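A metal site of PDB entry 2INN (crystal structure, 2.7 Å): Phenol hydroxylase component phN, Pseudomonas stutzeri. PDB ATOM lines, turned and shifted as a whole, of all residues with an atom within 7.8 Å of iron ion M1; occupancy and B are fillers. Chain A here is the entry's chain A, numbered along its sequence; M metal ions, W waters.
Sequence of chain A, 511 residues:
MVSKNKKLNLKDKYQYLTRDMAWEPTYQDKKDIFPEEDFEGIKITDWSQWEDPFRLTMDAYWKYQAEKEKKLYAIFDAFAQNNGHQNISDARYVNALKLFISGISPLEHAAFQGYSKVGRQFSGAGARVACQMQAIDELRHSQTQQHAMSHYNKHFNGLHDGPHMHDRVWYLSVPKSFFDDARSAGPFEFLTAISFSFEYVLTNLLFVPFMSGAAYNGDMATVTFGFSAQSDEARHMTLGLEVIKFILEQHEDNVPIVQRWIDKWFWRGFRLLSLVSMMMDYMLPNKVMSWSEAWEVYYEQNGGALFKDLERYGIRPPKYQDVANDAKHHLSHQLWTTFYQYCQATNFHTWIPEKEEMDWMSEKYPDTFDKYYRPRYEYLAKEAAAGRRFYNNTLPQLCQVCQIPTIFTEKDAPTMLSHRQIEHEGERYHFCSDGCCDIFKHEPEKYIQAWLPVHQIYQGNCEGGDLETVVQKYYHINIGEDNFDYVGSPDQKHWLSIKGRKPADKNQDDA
Glu 199 touches iron ion M1 (OE1 to FE, 3.9 Å). OE1 of Glu 233 touches iron ion M1, at 3.9 Å. Within 4 Å of iron ion M1: Glu 108, Glu 138, His 141, Glu 199 and Glu 233.
OD2 of Asp 232 lies within hydrogen-bond range of NE2 of His 141 (3.1 Å). A ring nitrogen (ND1) of His 236 sits close to the side-chain carboxylate of Glu 138 (3.2 Å). The side-chain amide nitrogen (NE2) of Gln 145 sits at hydrogen-bond distance from the side-chain carboxylate (OE1) of Glu 108 (3.5 Å). OE1 of Glu 138 sits at hydrogen-bond distance from NE2 of Gln 134 (3.0 Å). The side-chain carboxylate (OE1) of Glu 199 lies close to the side-chain amide nitrogen (NE2) of Gln 134 (3.3 Å).
Water W2 lies within hydrogen-bond range of OE1 of Glu 108 (2.4 Å) and OE1 of Glu 233 (2.6 Å). Water W1 lies within hydrogen-bond range of the side-chain carboxylate (OE1) of Glu 138 (3.1 Å) and the side-chain carboxylate (OE1) of Glu 108 (3.2 Å).
Iron ion M1 is bound by water W1 (1.9 Å), the side-chain carboxylate (OE2) of Glu 138 (2.1 Å), the side-chain carboxylate (OE2) of Glu 108 (2.1 Å), a ring nitrogen (ND1) of His 141 (2.1 Å) and water W2 (2.5 Å). Slightly farther from iron ion M1 lies OE1 of Glu 108 (2.8 Å).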
ATOM      1  N   ILE A 104      18.170   4.012 -20.710  1.00  0.00           N
ATOM      2  CA  ILE A 104      17.831   3.002 -21.662  1.00  0.00           C
ATOM      3  C   ILE A 104      17.685   1.705 -20.948  1.00  0.00           C
ATOM      4  O   ILE A 104      16.772   0.923 -21.219  1.00  0.00           O
ATOM      5  CB  ILE A 104      18.865   2.928 -22.742  1.00  0.00           C
ATOM      6  CG1 ILE A 104      18.415   3.707 -23.970  1.00  0.00           C
ATOM      7  CG2 ILE A 104      19.098   1.471 -23.219  1.00  0.00           C
ATOM      8  CD1 ILE A 104      18.645   5.206 -23.925  1.00  0.00           C
ATOM      9  N   SER A 105      18.574   1.480 -19.992  1.00  0.00           N
ATOM     10  CA  SER A 105      18.677   0.221 -19.352  1.00  0.00           C
ATOM     11  C   SER A 105      17.386  -0.130 -18.578  1.00  0.00           C
ATOM     12  O   SER A 105      16.881  -1.209 -18.726  1.00  0.00           O
ATOM     13  CB  SER A 105      19.921   0.272 -18.504  1.00  0.00           C
ATOM     14  OG  SER A 105      20.252  -0.990 -18.053  1.00  0.00           O
ATOM     15  N   LEU A 107      14.494   0.600 -19.414  1.00  0.00           N
ATOM     16  CA  LEU A 107      13.557   0.111 -20.452  1.00  0.00           C
ATOM     17  C   LEU A 107      13.763  -1.411 -20.733  1.00  0.00           C
ATOM     18  O   LEU A 107      12.787  -2.176 -20.966  1.00  0.00           O
ATOM     19  CB  LEU A 107      13.726   0.918 -21.696  1.00  0.00           C
ATOM     20  CG  LEU A 107      12.955   2.188 -21.900  1.00  0.00           C
ATOM     21  CD1 LEU A 107      12.551   2.863 -20.596  1.00  0.00           C
ATOM     22  CD2 LEU A 107      13.793   3.111 -22.744  1.00  0.00           C
ATOM     23  N   GLU A 108      15.008  -1.859 -20.713  1.00  0.00           N
ATOM     24  CA  GLU A 108      15.247  -3.255 -20.844  1.00  0.00           C
ATOM     25  C   GLU A 108      14.297  -3.968 -19.885  1.00  0.00           C
ATOM     26  O   GLU A 108      13.579  -4.915 -20.268  1.00  0.00           O
ATOM     27  CB  GLU A 108      16.736  -3.662 -20.566  1.00  0.00           C
ATOM     28  CG  GLU A 108      17.741  -3.222 -21.675  1.00  0.00           C
ATOM     29  CD  GLU A 108      17.403  -3.631 -23.134  1.00  0.00           C
ATOM     30  OE1 GLU A 108      18.160  -3.240 -24.047  1.00  0.00           O
ATOM     31  OE2 GLU A 108      16.428  -4.339 -23.429  1.00  0.00           O
ATOM     32  N   HIS A 109      14.277  -3.504 -18.641  1.00  0.00           N
ATOM     33  CA  HIS A 109      13.513  -4.234 -17.627  1.00  0.00           C
ATOM     34  C   HIS A 109      12.004  -4.012 -17.802  1.00  0.00           C
ATOM     35  O   HIS A 109      11.175  -4.896 -17.578  1.00  0.00           O
ATOM     36  CB  HIS A 109      13.913  -3.768 -16.241  1.00  0.00           C
ATOM     37  CG  HIS A 109      13.884  -4.834 -15.240  1.00  0.00           C
ATOM     38  ND1 HIS A 109      14.913  -5.756 -15.114  1.00  0.00           N
ATOM     39  CD2 HIS A 109      13.007  -5.099 -14.228  1.00  0.00           C
ATOM     40  CE1 HIS A 109      14.656  -6.548 -14.069  1.00  0.00           C
ATOM     41  NE2 HIS A 109      13.496  -6.180 -13.527  1.00  0.00           N
ATOM     42  N   ALA A 111      10.474  -3.900 -20.554  1.00  0.00           N
ATOM     43  CA  ALA A 111      10.231  -4.920 -21.574  1.00  0.00           C
ATOM     44  C   ALA A 111      10.146  -6.398 -20.986  1.00  0.00           C
ATOM     45  O   ALA A 111       9.155  -7.129 -21.214  1.00  0.00           O
ATOM     46  CB  ALA A 111      11.275  -4.782 -22.689  1.00  0.00           C
ATOM     47  N   PHE A 112      11.153  -6.820 -20.211  1.00  0.00           N
ATOM     48  CA  PHE A 112      11.041  -8.096 -19.526  1.00  0.00           C
ATOM     49  C   PHE A 112       9.667  -8.234 -18.904  1.00  0.00           C
ATOM     50  O   PHE A 112       9.055  -9.256 -19.043  1.00  0.00           O
ATOM     51  CB  PHE A 112      12.086  -8.167 -18.409  1.00  0.00           C
ATOM     52  CG  PHE A 112      11.749  -9.164 -17.344  1.00  0.00           C
ATOM     53  CD1 PHE A 112      11.656 -10.493 -17.631  1.00  0.00           C
ATOM     54  CD2 PHE A 112      11.512  -8.751 -16.070  1.00  0.00           C
ATOM     55  CE1 PHE A 112      11.363 -11.412 -16.652  1.00  0.00           C
ATOM     56  CE2 PHE A 112      11.193  -9.642 -15.114  1.00  0.00           C
ATOM     57  CZ  PHE A 112      11.120 -10.985 -15.394  1.00  0.00           C
ATOM     58  N   GLN A 134      11.196 -13.487 -25.676  1.00  0.00           N
ATOM     59  CA  GLN A 134      11.661 -12.139 -25.762  1.00  0.00           C
ATOM     60  C   GLN A 134      11.771 -11.606 -24.328  1.00  0.00           C
ATOM     61  O   GLN A 134      12.823 -11.191 -23.858  1.00  0.00           O
ATOM     62  CB  GLN A 134      10.797 -11.274 -26.643  1.00  0.00           C
ATOM     63  CG  GLN A 134      11.304  -9.909 -26.552  1.00  0.00           C
ATOM     64  CD  GLN A 134      11.331  -9.156 -27.865  1.00  0.00           C
ATOM     65  OE1 GLN A 134      11.006  -9.718 -28.907  1.00  0.00           O
ATOM     66  NE2 GLN A 134      11.785  -7.863 -27.840  1.00  0.00           N
ATOM     67  N   ASP A 137      14.902 -12.660 -22.784  1.00  0.00           N
ATOM     68  CA  ASP A 137      16.016 -12.000 -23.363  1.00  0.00           C
ATOM     69  C   ASP A 137      16.164 -10.617 -22.740  1.00  0.00           C
ATOM     70  O   ASP A 137      17.269 -10.113 -22.529  1.00  0.00           O
ATOM     71  CB  ASP A 137      15.789 -11.767 -24.872  1.00  0.00           C
ATOM     72  CG  ASP A 137      15.990 -13.014 -25.712  1.00  0.00           C
ATOM     73  OD1 ASP A 137      16.795 -13.897 -25.311  1.00  0.00           O
ATOM     74  OD2 ASP A 137      15.268 -13.066 -26.770  1.00  0.00           O
ATOM     75  N   GLU A 138      15.039  -9.955 -22.528  1.00  0.00           N
ATOM     76  CA  GLU A 138      15.095  -8.551 -22.097  1.00  0.00           C
ATOM     77  C   GLU A 138      15.549  -8.560 -20.674  1.00  0.00           C
ATOM     78  O   GLU A 138      16.258  -7.653 -20.262  1.00  0.00           O
ATOM     79  CB  GLU A 138      13.796  -7.740 -22.311  1.00  0.00           C
ATOM     80  CG  GLU A 138      13.290  -7.719 -23.770  1.00  0.00           C
ATOM     81  CD  GLU A 138      14.205  -7.001 -24.752  1.00  0.00           C
ATOM     82  OE1 GLU A 138      13.811  -6.806 -25.950  1.00  0.00           O
ATOM     83  OE2 GLU A 138      15.377  -6.712 -24.381  1.00  0.00           O
ATOM     84  N   LEU A 139      15.258  -9.639 -19.967  1.00  0.00           N
ATOM     85  CA  LEU A 139      15.745  -9.724 -18.603  1.00  0.00           C
ATOM     86  C   LEU A 139      17.254  -9.898 -18.708  1.00  0.00           C
ATOM     87  O   LEU A 139      17.986  -9.194 -18.014  1.00  0.00           O
ATOM     88  CB  LEU A 139      15.150 -10.899 -17.886  1.00  0.00           C
ATOM     89  CG  LEU A 139      15.642 -11.109 -16.485  1.00  0.00           C
ATOM     90  CD1 LEU A 139      15.130 -10.063 -15.452  1.00  0.00           C
ATOM     91  CD2 LEU A 139      15.302 -12.503 -16.056  1.00  0.00           C
ATOM     92  N   ARG A 140      17.740 -10.829 -19.556  1.00  0.00           N
ATOM     93  CA  ARG A 140      19.156 -10.848 -19.826  1.00  0.00           C
ATOM     94  C   ARG A 140      19.786  -9.514 -20.154  1.00  0.00           C
ATOM     95  O   ARG A 140      20.833  -9.166 -19.587  1.00  0.00           O
ATOM     96  CB  ARG A 140      19.450 -11.754 -20.963  1.00  0.00           C
ATOM     97  CG  ARG A 140      20.886 -11.669 -21.395  1.00  0.00           C
ATOM     98  CD  ARG A 140      21.425 -12.829 -22.247  1.00  0.00           C
ATOM     99  NE  ARG A 140      21.994 -12.220 -23.442  1.00  0.00           N
ATOM    100  CZ  ARG A 140      23.235 -12.431 -23.948  1.00  0.00           C
ATOM    101  NH1 ARG A 140      24.121 -13.257 -23.371  1.00  0.00           N
ATOM    102  NH2 ARG A 140      23.577 -11.821 -25.077  1.00  0.00           N
ATOM    103  N   HIS A 141      19.233  -8.795 -21.116  1.00  0.00           N
ATOM    104  CA  HIS A 141      19.723  -7.487 -21.423  1.00  0.00           C
ATOM    105  C   HIS A 141      19.814  -6.715 -20.116  1.00  0.00           C
ATOM    106  O   HIS A 141      20.834  -6.083 -19.860  1.00  0.00           O
ATOM    107  CB  HIS A 141      18.794  -6.756 -22.406  1.00  0.00           C
ATOM    108  CG  HIS A 141      18.843  -7.371 -23.761  1.00  0.00           C
ATOM    109  ND1 HIS A 141      18.248  -6.800 -24.873  1.00  0.00           N
ATOM    110  CD2 HIS A 141      19.471  -8.512 -24.175  1.00  0.00           C
ATOM    111  CE1 HIS A 141      18.507  -7.567 -25.934  1.00  0.00           C
ATOM    112  NE2 HIS A 141      19.264  -8.598 -25.545  1.00  0.00           N
ATOM    113  N   SER A 142      18.764  -6.726 -19.281  1.00  0.00           N
ATOM    114  CA  SER A 142      18.767  -5.836 -18.119  1.00  0.00           C
ATOM    115  C   SER A 142      19.854  -6.199 -17.113  1.00  0.00           C
ATOM    116  O   SER A 142      20.657  -5.370 -16.727  1.00  0.00           O
ATOM    117  CB  SER A 142      17.406  -5.798 -17.457  1.00  0.00           C
ATOM    118  OG  SER A 142      17.358  -5.001 -16.284  1.00  0.00           O
ATOM    119  N   GLN A 145      23.543  -5.443 -18.617  1.00  0.00           N
ATOM    120  CA  GLN A 145      23.931  -4.073 -18.507  1.00  0.00           C
ATOM    121  C   GLN A 145      24.310  -3.677 -17.086  1.00  0.00           C
ATOM    122  O   GLN A 145      25.160  -2.861 -16.876  1.00  0.00           O
ATOM    123  CB  GLN A 145      22.778  -3.238 -19.004  1.00  0.00           C
ATOM    124  CG  GLN A 145      22.348  -3.793 -20.331  1.00  0.00           C
ATOM    125  CD  GLN A 145      21.370  -2.990 -21.091  1.00  0.00           C
ATOM    126  OE1 GLN A 145      20.827  -2.037 -20.614  1.00  0.00           O
ATOM    127  NE2 GLN A 145      21.171  -3.360 -22.329  1.00  0.00           N
ATOM    128  N   PHE A 198       9.547  -0.100 -32.084  1.00  0.00           N
ATOM    129  CA  PHE A 198      10.823   0.182 -31.428  1.00  0.00           C
ATOM    130  C   PHE A 198      11.816  -0.884 -31.860  1.00  0.00           C
ATOM    131  O   PHE A 198      12.830  -0.571 -32.447  1.00  0.00           O
ATOM    132  CB  PHE A 198      10.554   0.015 -29.975  1.00  0.00           C
ATOM    133  CG  PHE A 198      11.616   0.504 -28.999  1.00  0.00           C
ATOM    134  CD1 PHE A 198      11.876   1.887 -28.826  1.00  0.00           C
ATOM    135  CD2 PHE A 198      12.159  -0.445 -28.045  1.00  0.00           C
ATOM    136  CE1 PHE A 198      12.739   2.335 -27.764  1.00  0.00           C
ATOM    137  CE2 PHE A 198      13.047  -0.055 -27.004  1.00  0.00           C
ATOM    138  CZ  PHE A 198      13.338   1.319 -26.850  1.00  0.00           C
ATOM    139  N   GLU A 199      11.488  -2.145 -31.608  1.00  0.00           N
ATOM    140  CA  GLU A 199      12.398  -3.188 -31.932  1.00  0.00           C
ATOM    141  C   GLU A 199      12.615  -3.379 -33.446  1.00  0.00           C
ATOM    142  O   GLU A 199      13.654  -3.860 -33.870  1.00  0.00           O
ATOM    143  CB  GLU A 199      12.236  -4.462 -31.036  1.00  0.00           C
ATOM    144  CG  GLU A 199      12.474  -4.226 -29.467  1.00  0.00           C
ATOM    145  CD  GLU A 199      13.481  -5.187 -28.741  1.00  0.00           C
ATOM    146  OE1 GLU A 199      13.643  -5.173 -27.503  1.00  0.00           O
ATOM    147  OE2 GLU A 199      14.166  -5.972 -29.372  1.00  0.00           O
ATOM    148  N   THR A 203      15.010   0.300 -33.909  1.00  0.00           N
ATOM    149  CA  THR A 203      15.992  -0.349 -33.109  1.00  0.00           C
ATOM    150  C   THR A 203      17.486   0.036 -33.455  1.00  0.00           C
ATOM    151  O   THR A 203      18.331   0.211 -32.551  1.00  0.00           O
ATOM    152  CB  THR A 203      15.805  -1.867 -33.201  1.00  0.00           C
ATOM    153  OG1 THR A 203      16.554  -2.537 -32.193  1.00  0.00           O
ATOM    154  CG2 THR A 203      16.340  -2.375 -34.508  1.00  0.00           C
ATOM    155  N   PHE A 207      20.573   1.536 -31.072  1.00  0.00           N
ATOM    156  CA  PHE A 207      21.468   0.460 -30.715  1.00  0.00           C
ATOM    157  C   PHE A 207      22.791   0.778 -31.332  1.00  0.00           C
ATOM    158  O   PHE A 207      23.749   0.971 -30.609  1.00  0.00           O
ATOM    159  CB  PHE A 207      20.923  -0.874 -31.245  1.00  0.00           C
ATOM    160  CG  PHE A 207      21.667  -2.119 -30.738  1.00  0.00           C
ATOM    161  CD1 PHE A 207      22.611  -2.805 -31.600  1.00  0.00           C
ATOM    162  CD2 PHE A 207      21.414  -2.630 -29.408  1.00  0.00           C
ATOM    163  CE1 PHE A 207      23.302  -4.007 -31.156  1.00  0.00           C
ATOM    164  CE2 PHE A 207      22.116  -3.819 -28.942  1.00  0.00           C
ATOM    165  CZ  PHE A 207      23.069  -4.514 -29.848  1.00  0.00           C
ATOM    166  N   PHE A 225      28.932  -6.248 -24.793  1.00  0.00           N
ATOM    167  CA  PHE A 225      27.617  -6.599 -24.411  1.00  0.00           C
ATOM    168  C   PHE A 225      26.875  -6.600 -25.805  1.00  0.00           C
ATOM    169  O   PHE A 225      26.052  -7.574 -26.120  1.00  0.00           O
ATOM    170  CB  PHE A 225      27.013  -5.627 -23.405  1.00  0.00           C
ATOM    171  CG  PHE A 225      25.556  -5.510 -23.605  1.00  0.00           C
ATOM    172  CD1 PHE A 225      24.660  -6.624 -23.235  1.00  0.00           C
ATOM    173  CD2 PHE A 225      24.998  -4.393 -24.331  1.00  0.00           C
ATOM    174  CE1 PHE A 225      23.224  -6.582 -23.444  1.00  0.00           C
ATOM    175  CE2 PHE A 225      23.515  -4.302 -24.592  1.00  0.00           C
ATOM    176  CZ  PHE A 225      22.624  -5.368 -24.119  1.00  0.00           C
ATOM    177  N   ALA A 229      24.620  -9.246 -27.776  1.00  0.00           N
ATOM    178  CA  ALA A 229      23.168  -8.977 -27.990  1.00  0.00           C
ATOM    179  C   ALA A 229      22.678  -9.082 -29.461  1.00  0.00           C
ATOM    180  O   ALA A 229      21.476  -9.114 -29.713  1.00  0.00           O
ATOM    181  CB  ALA A 229      22.751  -7.589 -27.479  1.00  0.00           C
ATOM    182  N   ASP A 232      20.390 -11.995 -30.197  1.00  0.00           N
ATOM    183  CA  ASP A 232      19.136 -11.657 -29.537  1.00  0.00           C
ATOM    184  C   ASP A 232      18.290 -10.741 -30.394  1.00  0.00           C
ATOM    185  O   ASP A 232      17.243 -11.157 -30.777  1.00  0.00           O
ATOM    186  CB  ASP A 232      19.412 -10.968 -28.233  1.00  0.00           C
ATOM    187  CG  ASP A 232      19.983 -11.892 -27.200  1.00  0.00           C
ATOM    188  OD1 ASP A 232      19.910 -13.144 -27.374  1.00  0.00           O
ATOM    189  OD2 ASP A 232      20.464 -11.336 -26.186  1.00  0.00           O
ATOM    190  N   GLU A 233      18.744  -9.534 -30.747  1.00  0.00           N
ATOM    191  CA  GLU A 233      17.987  -8.624 -31.582  1.00  0.00           C
ATOM    192  C   GLU A 233      17.504  -9.285 -32.917  1.00  0.00           C
ATOM    193  O   GLU A 233      16.390  -9.044 -33.369  1.00  0.00           O
ATOM    194  CB  GLU A 233      18.794  -7.361 -31.828  1.00  0.00           C
ATOM    195  CG  GLU A 233      19.300  -6.556 -30.547  1.00  0.00           C
ATOM    196  CD  GLU A 233      18.188  -5.991 -29.457  1.00  0.00           C
ATOM    197  OE1 GLU A 233      18.568  -5.067 -28.680  1.00  0.00           O
ATOM    198  OE2 GLU A 233      16.983  -6.445 -29.354  1.00  0.00           O
ATOM    199  N   HIS A 236      14.489 -10.561 -32.047  1.00  0.00           N
ATOM    200  CA  HIS A 236      13.449  -9.632 -31.680  1.00  0.00           C
ATOM    201  C   HIS A 236      12.892  -8.973 -32.918  1.00  0.00           C
ATOM    202  O   HIS A 236      11.695  -8.828 -32.993  1.00  0.00           O
ATOM    203  CB  HIS A 236      13.877  -8.657 -30.625  1.00  0.00           C
ATOM    204  CG  HIS A 236      14.415  -9.303 -29.394  1.00  0.00           C
ATOM    205  ND1 HIS A 236      14.960  -8.579 -28.334  1.00  0.00           N
ATOM    206  CD2 HIS A 236      14.543 -10.616 -29.046  1.00  0.00           C
ATOM    207  CE1 HIS A 236      15.371  -9.434 -27.398  1.00  0.00           C
ATOM    208  NE2 HIS A 236      15.126 -10.664 -27.806  1.00  0.00           N
HETATM  209 FE    FE M   1      16.738  -5.380 -25.217  1.00  0.00          FE
HETATM  210 FE    FE M   2      15.532  -6.490 -27.881  1.00  0.00          FE
HETATM  211  O   HOH W   1      15.372  -4.124 -25.462  1.00  0.00           O
HETATM  212  O   HOH W   2      18.394  -3.918 -26.350  1.00  0.00           O
